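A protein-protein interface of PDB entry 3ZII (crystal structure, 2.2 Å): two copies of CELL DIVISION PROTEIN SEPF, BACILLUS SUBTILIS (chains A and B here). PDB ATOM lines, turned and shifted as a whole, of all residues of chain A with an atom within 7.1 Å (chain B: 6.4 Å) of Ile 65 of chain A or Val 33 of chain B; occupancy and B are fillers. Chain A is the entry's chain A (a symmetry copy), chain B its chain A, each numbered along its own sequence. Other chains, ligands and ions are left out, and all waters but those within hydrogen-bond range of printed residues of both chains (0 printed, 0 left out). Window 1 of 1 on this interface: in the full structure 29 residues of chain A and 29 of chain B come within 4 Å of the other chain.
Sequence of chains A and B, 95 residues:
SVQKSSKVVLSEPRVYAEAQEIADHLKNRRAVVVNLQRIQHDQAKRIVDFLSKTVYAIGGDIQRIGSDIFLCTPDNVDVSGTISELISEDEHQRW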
ATOM      1  N   VAL A  32      22.168  24.998  19.666  1.00  0.00           N
ATOM      2  CA  VAL A  32      22.528  24.863  21.069  1.00  0.00           C
ATOM      3  C   VAL A  32      23.272  23.566  21.298  1.00  0.00           C
ATOM      4  O   VAL A  32      22.824  22.491  20.889  1.00  0.00           O
ATOM      5  CB  VAL A  32      21.287  24.893  22.031  1.00  0.00           C
ATOM      6  CG1 VAL A  32      21.735  24.960  23.486  1.00  0.00           C
ATOM      7  CG2 VAL A  32      20.354  26.050  21.713  1.00  0.00           C
ATOM      8  N   VAL A  33      24.419  23.660  21.954  1.00  0.00           N
ATOM      9  CA  VAL A  33      25.093  22.462  22.414  1.00  0.00           C
ATOM     10  C   VAL A  33      24.685  22.256  23.858  1.00  0.00           C
ATOM     11  O   VAL A  33      24.836  23.160  24.674  1.00  0.00           O
ATOM     12  CB  VAL A  33      26.619  22.599  22.327  1.00  0.00           C
ATOM     13  CG1 VAL A  33      27.276  21.382  22.930  1.00  0.00           C
ATOM     14  CG2 VAL A  33      27.059  22.775  20.875  1.00  0.00           C
ATOM     15  N   VAL A  34      24.147  21.080  24.163  1.00  0.00           N
ATOM     16  CA  VAL A  34      23.679  20.768  25.506  1.00  0.00           C
ATOM     17  C   VAL A  34      24.504  19.650  26.151  1.00  0.00           C
ATOM     18  O   VAL A  34      24.477  18.505  25.697  1.00  0.00           O
ATOM     19  CB  VAL A  34      22.221  20.312  25.482  1.00  0.00           C
ATOM     20  CG1 VAL A  34      21.669  20.335  26.887  1.00  0.00           C
ATOM     21  CG2 VAL A  34      21.406  21.209  24.555  1.00  0.00           C
ATOM     22  N   GLN A  63      20.578  15.588  18.054  1.00  0.00           N
ATOM     23  CA  GLN A  63      21.415  14.408  17.928  1.00  0.00           C
ATOM     24  C   GLN A  63      22.529  14.397  18.964  1.00  0.00           C
ATOM     25  O   GLN A  63      23.099  15.438  19.313  1.00  0.00           O
ATOM     26  CB  GLN A  63      22.011  14.303  16.516  1.00  0.00           C
ATOM     27  CG  GLN A  63      22.950  15.441  16.115  1.00  0.00           C
ATOM     28  CD  GLN A  63      22.985  15.643  14.614  1.00  0.00           C
ATOM     29  OE1 GLN A  63      22.255  16.479  14.061  1.00  0.00           O
ATOM     30  NE2 GLN A  63      23.814  14.858  13.939  1.00  0.00           N
ATOM     31  N   ARG A  64      22.830  13.203  19.452  1.00  0.00           N
ATOM     32  CA  ARG A  64      23.916  13.004  20.389  1.00  0.00           C
ATOM     33  C   ARG A  64      25.260  13.151  19.665  1.00  0.00           C
ATOM     34  O   ARG A  64      25.479  12.522  18.626  1.00  0.00           O
ATOM     35  CB  ARG A  64      23.781  11.616  20.997  1.00  0.00           C
ATOM     36  CG  ARG A  64      24.734  11.292  22.114  1.00  0.00           C
ATOM     37  CD  ARG A  64      24.208  10.066  22.827  1.00  0.00           C
ATOM     38  NE  ARG A  64      25.245   9.303  23.497  1.00  0.00           N
ATOM     39  CZ  ARG A  64      24.991   8.282  24.305  1.00  0.00           C
ATOM     40  NH1 ARG A  64      23.732   7.922  24.534  1.00  0.00           N
ATOM     41  NH2 ARG A  64      25.989   7.627  24.884  1.00  0.00           N
ATOM     42  N   ILE A  65      26.147  13.986  20.204  1.00  0.00           N
ATOM     43  CA  ILE A  65      27.483  14.159  19.616  1.00  0.00           C
ATOM     44  C   ILE A  65      28.620  13.598  20.493  1.00  0.00           C
ATOM     45  O   ILE A  65      29.782  13.574  20.089  1.00  0.00           O
ATOM     46  CB  ILE A  65      27.766  15.635  19.234  1.00  0.00           C
ATOM     47  CG1 ILE A  65      27.547  16.558  20.433  1.00  0.00           C
ATOM     48  CG2 ILE A  65      26.880  16.066  18.074  1.00  0.00           C
ATOM     49  CD1 ILE A  65      27.890  18.023  20.145  1.00  0.00           C
ATOM     50  N   GLY A  66      28.273  13.136  21.685  1.00  0.00           N
ATOM     51  CA  GLY A  66      29.234  12.501  22.571  1.00  0.00           C
ATOM     52  C   GLY A  66      28.483  11.981  23.780  1.00  0.00           C
ATOM     53  O   GLY A  66      27.256  12.071  23.830  1.00  0.00           O
ATOM     54  N   SER A  67      29.205  11.437  24.753  1.00  0.00           N
ATOM     55  CA  SER A  67      28.563  10.953  25.969  1.00  0.00           C
ATOM     56  C   SER A  67      27.947  12.124  26.741  1.00  0.00           C
ATOM     57  O   SER A  67      28.640  13.082  27.087  1.00  0.00           O
ATOM     58  CB  SER A  67      29.567  10.192  26.842  1.00  0.00           C
ATOM     59  OG  SER A  67      30.709  10.986  27.120  1.00  0.00           O
ATOM     60  N   ASP A  68      26.640  12.054  26.973  1.00  0.00           N
ATOM     61  CA  ASP A  68      25.902  13.120  27.662  1.00  0.00           C
ATOM     62  C   ASP A  68      25.878  14.478  26.940  1.00  0.00           C
ATOM     63  O   ASP A  68      25.499  15.485  27.534  1.00  0.00           O
ATOM     64  CB  ASP A  68      26.418  13.323  29.096  1.00  0.00           C
ATOM     65  CG  ASP A  68      26.224  12.096  29.975  1.00  0.00           C
ATOM     66  OD1 ASP A  68      25.355  11.254  29.653  1.00  0.00           O
ATOM     67  OD2 ASP A  68      26.944  11.986  30.996  1.00  0.00           O
ATOM     68  N   ILE A  69      26.267  14.523  25.672  1.00  0.00           N
ATOM     69  CA  ILE A  69      26.197  15.794  24.957  1.00  0.00           C
ATOM     70  C   ILE A  69      25.438  15.735  23.618  1.00  0.00           C
ATOM     71  O   ILE A  69      25.605  14.818  22.810  1.00  0.00           O
ATOM     72  CB  ILE A  69      27.585  16.484  24.847  1.00  0.00           C
ATOM     73  CG1 ILE A  69      27.527  17.700  23.926  1.00  0.00           C
ATOM     74  CG2 ILE A  69      28.636  15.516  24.385  1.00  0.00           C
ATOM     75  CD1 ILE A  69      28.861  18.379  23.806  1.00  0.00           C
ATOM     76  N   PHE A  70      24.577  16.729  23.421  1.00  0.00           N
ATOM     77  CA  PHE A  70      23.662  16.750  22.302  1.00  0.00           C
ATOM     78  C   PHE A  70      23.776  18.056  21.532  1.00  0.00           C
ATOM     79  O   PHE A  70      24.111  19.100  22.098  1.00  0.00           O
ATOM     80  CB  PHE A  70      22.239  16.502  22.803  1.00  0.00           C
ATOM     81  CG  PHE A  70      22.028  15.096  23.316  1.00  0.00           C
ATOM     82  CD1 PHE A  70      22.505  14.717  24.567  1.00  0.00           C
ATOM     83  CD2 PHE A  70      21.370  14.150  22.541  1.00  0.00           C
ATOM     84  CE1 PHE A  70      22.327  13.424  25.033  1.00  0.00           C
ATOM     85  CE2 PHE A  70      21.188  12.852  23.002  1.00  0.00           C
ATOM     86  CZ  PHE A  70      21.673  12.485  24.249  1.00  0.00           C
ATOM     87  N   LEU A  71      23.553  17.985  20.228  1.00  0.00           N
ATOM     88  CA  LEU A  71      23.501  19.188  19.410  1.00  0.00           C
ATOM     89  C   LEU A  71      22.058  19.365  18.980  1.00  0.00           C
ATOM     90  O   LEU A  71      21.502  18.489  18.314  1.00  0.00           O
ATOM     91  CB  LEU A  71      24.404  19.060  18.184  1.00  0.00           C
ATOM     92  CG  LEU A  71      24.311  20.176  17.124  1.00  0.00           C
ATOM     93  CD1 LEU A  71      24.786  21.522  17.667  1.00  0.00           C
ATOM     94  CD2 LEU A  71      25.097  19.820  15.870  1.00  0.00           C
ATOM     95  N   CYS A  72      21.446  20.471  19.399  1.00  0.00           N
ATOM     96  CA  CYS A  72      20.090  20.819  18.987  1.00  0.00           C
ATOM     97  C   CYS A  72      20.152  21.984  18.022  1.00  0.00           C
ATOM     98  O   CYS A  72      20.802  22.995  18.293  1.00  0.00           O
ATOM     99  CB  CYS A  72      19.214  21.222  20.185  1.00  0.00           C
ATOM    100  SG  CYS A  72      19.172  20.054  21.536  1.00  0.00           S
ATOM    101  N   VAL A  79      23.161  20.199   9.473  1.00  0.00           N
ATOM    102  CA  VAL A  79      24.209  19.370  10.069  1.00  0.00           C
ATOM    103  C   VAL A  79      24.689  18.287   9.093  1.00  0.00           C
ATOM    104  O   VAL A  79      23.882  17.568   8.504  1.00  0.00           O
ATOM    105  CB  VAL A  79      23.735  18.704  11.383  1.00  0.00           C
ATOM    106  CG1 VAL A  79      24.848  17.865  11.998  1.00  0.00           C
ATOM    107  CG2 VAL A  79      23.243  19.748  12.380  1.00  0.00           C
ATOM    108  N   ILE A  83      29.210  11.262  13.689  1.00  0.00           N
ATOM    109  CA  ILE A  83      29.938  10.807  14.871  1.00  0.00           C
ATOM    110  C   ILE A  83      29.286   9.522  15.386  1.00  0.00           C
ATOM    111  O   ILE A  83      28.114   9.530  15.768  1.00  0.00           O
ATOM    112  CB  ILE A  83      29.931  11.857  16.001  1.00  0.00           C
ATOM    113  CG1 ILE A  83      30.740  13.092  15.591  1.00  0.00           C
ATOM    114  CG2 ILE A  83      30.514  11.259  17.271  1.00  0.00           C
ATOM    115  CD1 ILE A  83      30.510  14.317  16.472  1.00  0.00           C
ATOM    116  N   SER A  84      30.046   8.427  15.381  1.00  0.00           N
ATOM    117  CA  SER A  84      29.541   7.109  15.760  1.00  0.00           C
ATOM    118  C   SER A  84      29.681   6.895  17.267  1.00  0.00           C
ATOM    119  O   SER A  84      30.387   7.650  17.941  1.00  0.00           O
ATOM    120  CB  SER A  84      30.306   6.013  15.008  1.00  0.00           C
ATOM    121  OG  SER A  84      31.641   5.911  15.478  1.00  0.00           O
ATOM    122  N   VAL B   8      26.830  23.139  10.264  1.00  0.00           N
ATOM    123  CA  VAL B   8      27.691  22.552  11.281  1.00  0.00           C
ATOM    124  C   VAL B   8      28.147  21.181  10.789  1.00  0.00           C
ATOM    125  O   VAL B   8      27.329  20.355  10.382  1.00  0.00           O
ATOM    126  CB  VAL B   8      26.973  22.404  12.639  1.00  0.00           C
ATOM    127  CG1 VAL B   8      27.919  21.864  13.681  1.00  0.00           C
ATOM    128  CG2 VAL B   8      26.407  23.746  13.099  1.00  0.00           C
ATOM    129  N   VAL B   9      29.454  20.957  10.809  1.00  0.00           N
ATOM    130  CA  VAL B   9      30.025  19.682  10.404  1.00  0.00           C
ATOM    131  C   VAL B   9      30.439  18.875  11.626  1.00  0.00           C
ATOM    132  O   VAL B   9      31.088  19.394  12.547  1.00  0.00           O
ATOM    133  CB  VAL B   9      31.247  19.888   9.490  1.00  0.00           C
ATOM    134  CG1 VAL B   9      31.798  18.552   9.000  1.00  0.00           C
ATOM    135  CG2 VAL B   9      30.878  20.785   8.318  1.00  0.00           C
ATOM    136  N   LEU B  10      30.047  17.604  11.647  1.00  0.00           N
ATOM    137  CA  LEU B  10      30.470  16.697  12.705  1.00  0.00           C
ATOM    138  C   LEU B  10      31.673  15.914  12.224  1.00  0.00           C
ATOM    139  O   LEU B  10      31.680  15.399  11.109  1.00  0.00           O
ATOM    140  CB  LEU B  10      29.357  15.723  13.072  1.00  0.00           C
ATOM    141  CG  LEU B  10      28.000  16.296  13.466  1.00  0.00           C
ATOM    142  CD1 LEU B  10      27.121  15.154  13.965  1.00  0.00           C
ATOM    143  CD2 LEU B  10      28.137  17.370  14.530  1.00  0.00           C
ATOM    144  N   SER B  11      32.687  15.815  13.075  1.00  0.00           N
ATOM    145  CA  SER B  11      33.917  15.145  12.709  1.00  0.00           C
ATOM    146  C   SER B  11      34.385  14.205  13.817  1.00  0.00           C
ATOM    147  O   SER B  11      34.383  14.562  14.991  1.00  0.00           O
ATOM    148  CB  SER B  11      34.998  16.179  12.393  1.00  0.00           C
ATOM    149  OG  SER B  11      36.270  15.558  12.297  1.00  0.00           O
ATOM    150  N   GLU B  12      34.770  12.995  13.428  1.00  0.00           N
ATOM    151  CA  GLU B  12      35.285  12.000  14.359  1.00  0.00           C
ATOM    152  C   GLU B  12      36.552  11.419  13.739  1.00  0.00           C
ATOM    153  O   GLU B  12      36.517  10.347  13.144  1.00  0.00           O
ATOM    154  CB  GLU B  12      34.240  10.896  14.591  1.00  0.00           C
ATOM    155  CG  GLU B  12      34.658   9.840  15.608  1.00  0.00           C
ATOM    156  CD  GLU B  12      33.697   8.657  15.690  1.00  0.00           C
ATOM    157  OE1 GLU B  12      32.770   8.541  14.849  1.00  0.00           O
ATOM    158  OE2 GLU B  12      33.877   7.832  16.611  1.00  0.00           O
ATOM    159  N   ILE B  22      39.521  19.269   8.742  1.00  0.00           N
ATOM    160  CA  ILE B  22      38.667  20.179   9.509  1.00  0.00           C
ATOM    161  C   ILE B  22      38.965  21.643   9.177  1.00  0.00           C
ATOM    162  O   ILE B  22      38.066  22.484   9.168  1.00  0.00           O
ATOM    163  CB  ILE B  22      38.839  19.917  11.028  1.00  0.00           C
ATOM    164  CG1 ILE B  22      38.124  18.629  11.417  1.00  0.00           C
ATOM    165  CG2 ILE B  22      38.353  21.083  11.867  1.00  0.00           C
ATOM    166  CD1 ILE B  22      38.580  18.073  12.728  1.00  0.00           C
ATOM    167  N   ALA B  31      31.168  25.920  11.174  1.00  0.00           N
ATOM    168  CA  ALA B  31      31.503  25.397  12.496  1.00  0.00           C
ATOM    169  C   ALA B  31      31.699  23.891  12.417  1.00  0.00           C
ATOM    170  O   ALA B  31      31.028  23.208  11.636  1.00  0.00           O
ATOM    171  CB  ALA B  31      30.407  25.723  13.499  1.00  0.00           C
ATOM    172  N   VAL B  32      32.624  23.375  13.224  1.00  0.00           N
ATOM    173  CA  VAL B  32      32.898  21.946  13.245  1.00  0.00           C
ATOM    174  C   VAL B  32      32.891  21.431  14.668  1.00  0.00           C
ATOM    175  O   VAL B  32      33.550  21.985  15.552  1.00  0.00           O
ATOM    176  CB  VAL B  32      34.280  21.573  12.596  1.00  0.00           C
ATOM    177  CG1 VAL B  32      34.418  20.062  12.457  1.00  0.00           C
ATOM    178  CG2 VAL B  32      34.469  22.246  11.246  1.00  0.00           C
ATOM    179  N   VAL B  33      32.139  20.365  14.896  1.00  0.00           N
ATOM    180  CA  VAL B  33      32.235  19.668  16.164  1.00  0.00           C
ATOM    181  C   VAL B  33      33.194  18.515  15.959  1.00  0.00           C
ATOM    182  O   VAL B  33      33.003  17.709  15.052  1.00  0.00           O
ATOM    183  CB  VAL B  33      30.873  19.126  16.620  1.00  0.00           C
ATOM    184  CG1 VAL B  33      31.043  18.305  17.874  1.00  0.00           C
ATOM    185  CG2 VAL B  33      29.895  20.274  16.866  1.00  0.00           C
ATOM    186  N   VAL B  34      34.235  18.452  16.782  1.00  0.00           N
ATOM    187  CA  VAL B  34      35.251  17.416  16.668  1.00  0.00           C
ATOM    188  C   VAL B  34      35.257  16.487  17.887  1.00  0.00           C
ATOM    189  O   VAL B  34      35.577  16.910  18.999  1.00  0.00           O
ATOM    190  CB  VAL B  34      36.644  18.030  16.547  1.00  0.00           C
ATOM    191  CG1 VAL B  34      37.618  16.971  16.086  1.00  0.00           C
ATOM    192  CG2 VAL B  34      36.616  19.210  15.581  1.00  0.00           C
ATOM    193  N   ASN B  35      34.904  15.227  17.672  1.00  0.00           N
ATOM    194  CA  ASN B  35      34.953  14.229  18.723  1.00  0.00           C
ATOM    195  C   ASN B  35      36.223  13.372  18.595  1.00  0.00           C
ATOM    196  O   ASN B  35      36.374  12.603  17.649  1.00  0.00           O
ATOM    197  CB  ASN B  35      33.698  13.353  18.686  1.00  0.00           C
ATOM    198  CG  ASN B  35      33.582  12.453  19.898  1.00  0.00           C
ATOM    199  OD1 ASN B  35      34.558  11.833  20.306  1.00  0.00           O
ATOM    200  ND2 ASN B  35      32.387  12.395  20.502  1.00  0.00           N
ATOM    201  N   GLN B  37      37.325  10.889  20.405  1.00  0.00           N
ATOM    202  CA  GLN B  37      37.232   9.616  21.135  1.00  0.00           C
ATOM    203  C   GLN B  37      38.041   8.458  20.504  1.00  0.00           C
ATOM    204  O   GLN B  37      38.374   7.492  21.186  1.00  0.00           O
ATOM    205  CB  GLN B  37      35.763   9.196  21.321  1.00  0.00           C
ATOM    206  CG  GLN B  37      35.070   8.755  20.024  1.00  0.00           C
ATOM    207  CD  GLN B  37      33.558   8.541  20.179  1.00  0.00           C
ATOM    208  OE1 GLN B  37      32.986   8.791  21.237  1.00  0.00           O
ATOM    209  NE2 GLN B  37      32.916   8.076  19.115  1.00  0.00           N
ATOM    210  N   ILE B  65      33.985  21.237  24.667  1.00  0.00           N
ATOM    211  CA  ILE B  65      32.582  21.230  25.104  1.00  0.00           C
ATOM    212  C   ILE B  65      32.187  19.966  25.891  1.00  0.00           C
ATOM    213  O   ILE B  65      31.077  19.861  26.412  1.00  0.00           O
ATOM    214  CB  ILE B  65      31.604  21.467  23.925  1.00  0.00           C
ATOM    215  CG1 ILE B  65      31.855  20.464  22.800  1.00  0.00           C
ATOM    216  CG2 ILE B  65      31.737  22.889  23.397  1.00  0.00           C
ATOM    217  CD1 ILE B  65      30.866  20.591  21.636  1.00  0.00           C
ATOM    218  N   ILE B  69      35.696  16.195  23.304  1.00  0.00           N
ATOM    219  CA  ILE B  69      34.971  16.880  22.237  1.00  0.00           C
ATOM    220  C   ILE B  69      35.132  18.412  22.234  1.00  0.00           C
ATOM    221  O   ILE B  69      35.066  19.080  23.269  1.00  0.00           O
ATOM    222  CB  ILE B  69      33.491  16.417  22.140  1.00  0.00           C
ATOM    223  CG1 ILE B  69      32.702  17.284  21.163  1.00  0.00           C
ATOM    224  CG2 ILE B  69      32.836  16.408  23.492  1.00  0.00           C
ATOM    225  CD1 ILE B  69      31.268  16.853  21.058  1.00  0.00           C
ATOM    226  N   PHE B  70      35.373  18.944  21.040  1.00  0.00           N
ATOM    227  CA  PHE B  70      35.713  20.339  20.869  1.00  0.00           C
ATOM    228  C   PHE B  70      34.801  20.999  19.848  1.00  0.00           C
ATOM    229  O   PHE B  70      34.306  20.348  18.923  1.00  0.00           O
ATOM    230  CB  PHE B  70      37.188  20.460  20.484  1.00  0.00           C
ATOM    231  CG  PHE B  70      38.126  20.074  21.603  1.00  0.00           C
ATOM    232  CD1 PHE B  70      38.347  18.737  21.917  1.00  0.00           C
ATOM    233  CD2 PHE B  70      38.773  21.048  22.354  1.00  0.00           C
ATOM    234  CE1 PHE B  70      39.195  18.380  22.954  1.00  0.00           C
ATOM    235  CE2 PHE B  70      39.624  20.697  23.394  1.00  0.00           C
ATOM    236  CZ  PHE B  70      39.832  19.360  23.700  1.00  0.00           C
ATOM    237  N   LEU B  71      34.531  22.280  20.049  1.00  0.00           N
ATOM    238  CA  LEU B  71      33.782  23.051  19.068  1.00  0.00           C
ATOM    239  C   LEU B  71      34.755  24.032  18.443  1.00  0.00           C
ATOM    240  O   LEU B  71      35.328  24.865  19.148  1.00  0.00           O
ATOM    241  CB  LEU B  71      32.625  23.804  19.726  1.00  0.00           C
ATOM    242  CG  LEU B  71      31.855  24.812  18.849  1.00  0.00           C
ATOM    243  CD1 LEU B  71      31.113  24.126  17.705  1.00  0.00           C
ATOM    244  CD2 LEU B  71      30.879  25.636  19.677  1.00  0.00           C
ATOM    245  N   CYS B  72      34.971  23.902  17.136  1.00  0.00           N
ATOM    246  CA  CYS B  72      35.808  24.831  16.383  1.00  0.00           C
ATOM    247  C   CYS B  72      34.924  25.689  15.505  1.00  0.00           C
ATOM    248  O   CYS B  72      34.070  25.180  14.777  1.00  0.00           O
ATOM    249  CB  CYS B  72      36.819  24.094  15.490  1.00  0.00           C
ATOM    250  SG  CYS B  72      37.831  22.875  16.314  1.00  0.00           S
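The side-chain amide nitrogen of Gln 37 of chain B sits at hydrogen-bond distance from the backbone carbonyl oxygen of Ser 84 of chain A.
OE1 of Glu 12 of chain B sits at hydrogen-bond distance from N of Ser 84 of chain A, at 2.8 Å.
The side-chain amide nitrogen (ND2) of Asn 35 of chain B is in hydrogen-bond range of the backbone carbonyl oxygen (O) of Ile 65 of chain A, at 2.9 Å.
The backbone carbonyl oxygen of Ser 11 of chain B is in hydrogen-bond range of the backbone NH of Asn 35 of chain B.
The backbone NH of Gln 37 of chain B lies within hydrogen-bond range of the side-chain amide oxygen of Asn 35 of chain B, 2.9 Å away.
The side-chain carboxylate (OE2) of Glu 12 of chain B is in hydrogen-bond range of the side-chain amide nitrogen (NE2) of Gln 37 of chain B (2.7 Å).
The backbone NH (N) of Ser 11 of chain B lies within hydrogen-bond range of the backbone carbonyl oxygen (O) of Val 33 of chain B (2.8 Å).
The guanidinium group (NE) of Arg 64 of chain A sits close to the backbone carbonyl oxygen (O) of Gly 66 of chain A (3.4 Å).
O of Gln 63 of chain A lies within hydrogen-bond range of N of Leu 71 of chain A, 2.7 Å away.
Ile 65 of chain B touches Val 33 of chain A (CD1 to CG1, 3.9 Å).
CD1 of Ile 65 of chain A touches CD1 of Ile 69 of chain B (3.7 Å).
CA of Gly 66 of chain A touches ND2 of Asn 35 of chain B, 3.8 Å away.
CD1 of Ile 65 of chain B touches CD1 of Ile 69 of chain A (3.7 Å).
Ile 69 of chain A touches Ile 69 of chain B.
CA of Val 79 of chain A touches O of Val 8 of chain B, 3.3 Å away.
Ile 83 of chain A touches Leu 10 of chain B.
O of Ser 11 of chain B touches CG1 of Ile 83 of chain A, at 3.97 Å.
Glu 12 of chain B touches Ile 83 of chain A (OE1 to CA, 3.6 Å).
CG2 of Ile 83 of chain A touches ND2 of Asn 35 of chain B, 3.9 Å away.
Of the printed residues of chain B, Ile 65 of chain A touches Leu 10, Val 33, Asn 35 and Ile 69.
Of the printed residues of chain B, Val 79 of chain A touches Val 8 (3.3 Å) and Leu 10 (3.8 Å).
Of the printed residues of chain B, Ile 83 of chain A touches Leu 10 (3.9 Å), Ser 11 (3.97 Å), Glu 12 (3.6 Å) and Asn 35 (3.9 Å).
Printed residues of chain A within 4 Å of Leu 10 of chain B: Gln 63 (3.3 Å), Ile 65 (3.98 Å), Val 79 (3.8 Å) and Ile 83 (3.9 Å).
Of the printed residues of chain A, Ser 11 of chain B touches Ile 83.
Printed residues of chain A within 4 Å of Ile 65 of chain B: Val 33 and Ile 69.
The nearest printed residue of chain B that does not touch Ile 65 of chain A is Ile 65 of chain B (4.2 Å).
The nearest printed residue of chain B that does not touch Val 79 of chain A is Val 9 of chain B (5.5 Å).
Hydrophobic or aromatic side chains of chain A within 4 Å of the printed part of chain B: Val 33, Ile 65, Ile 69, Val 79 and Ile 83.
Of the 17 printed residues of chain B, 9 touch a printed residue of chain A.
Hydrophobic or aromatic side chains of chain B that line the printed part of chain A: Leu 10, Val 33, Ile 65 and Ile 69.
Among the printed residues, 17 pairs touch across the chains.
Among the printed residues, no Asp or Glu carboxylate lies within 4 Å of a Lys or Arg side-chain nitrogen of the other chain.
Val 33 of chain A touches Ile 65 of chain B, and with the chains exchanged Ile 65 of chain A touches Val 33 of chain B.
Ile 65 of chain A touches Ile 69 of chain B, and with the chains exchanged Ile 69 of chain A touches Ile 65 of chain B.
Ile 69 of chain B touches its own counterpart, Ile 69 of chain A.
Of the 17 pairs that touch across the chains among the printed residues, 5 have their exchanged pair printed and touching as well.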
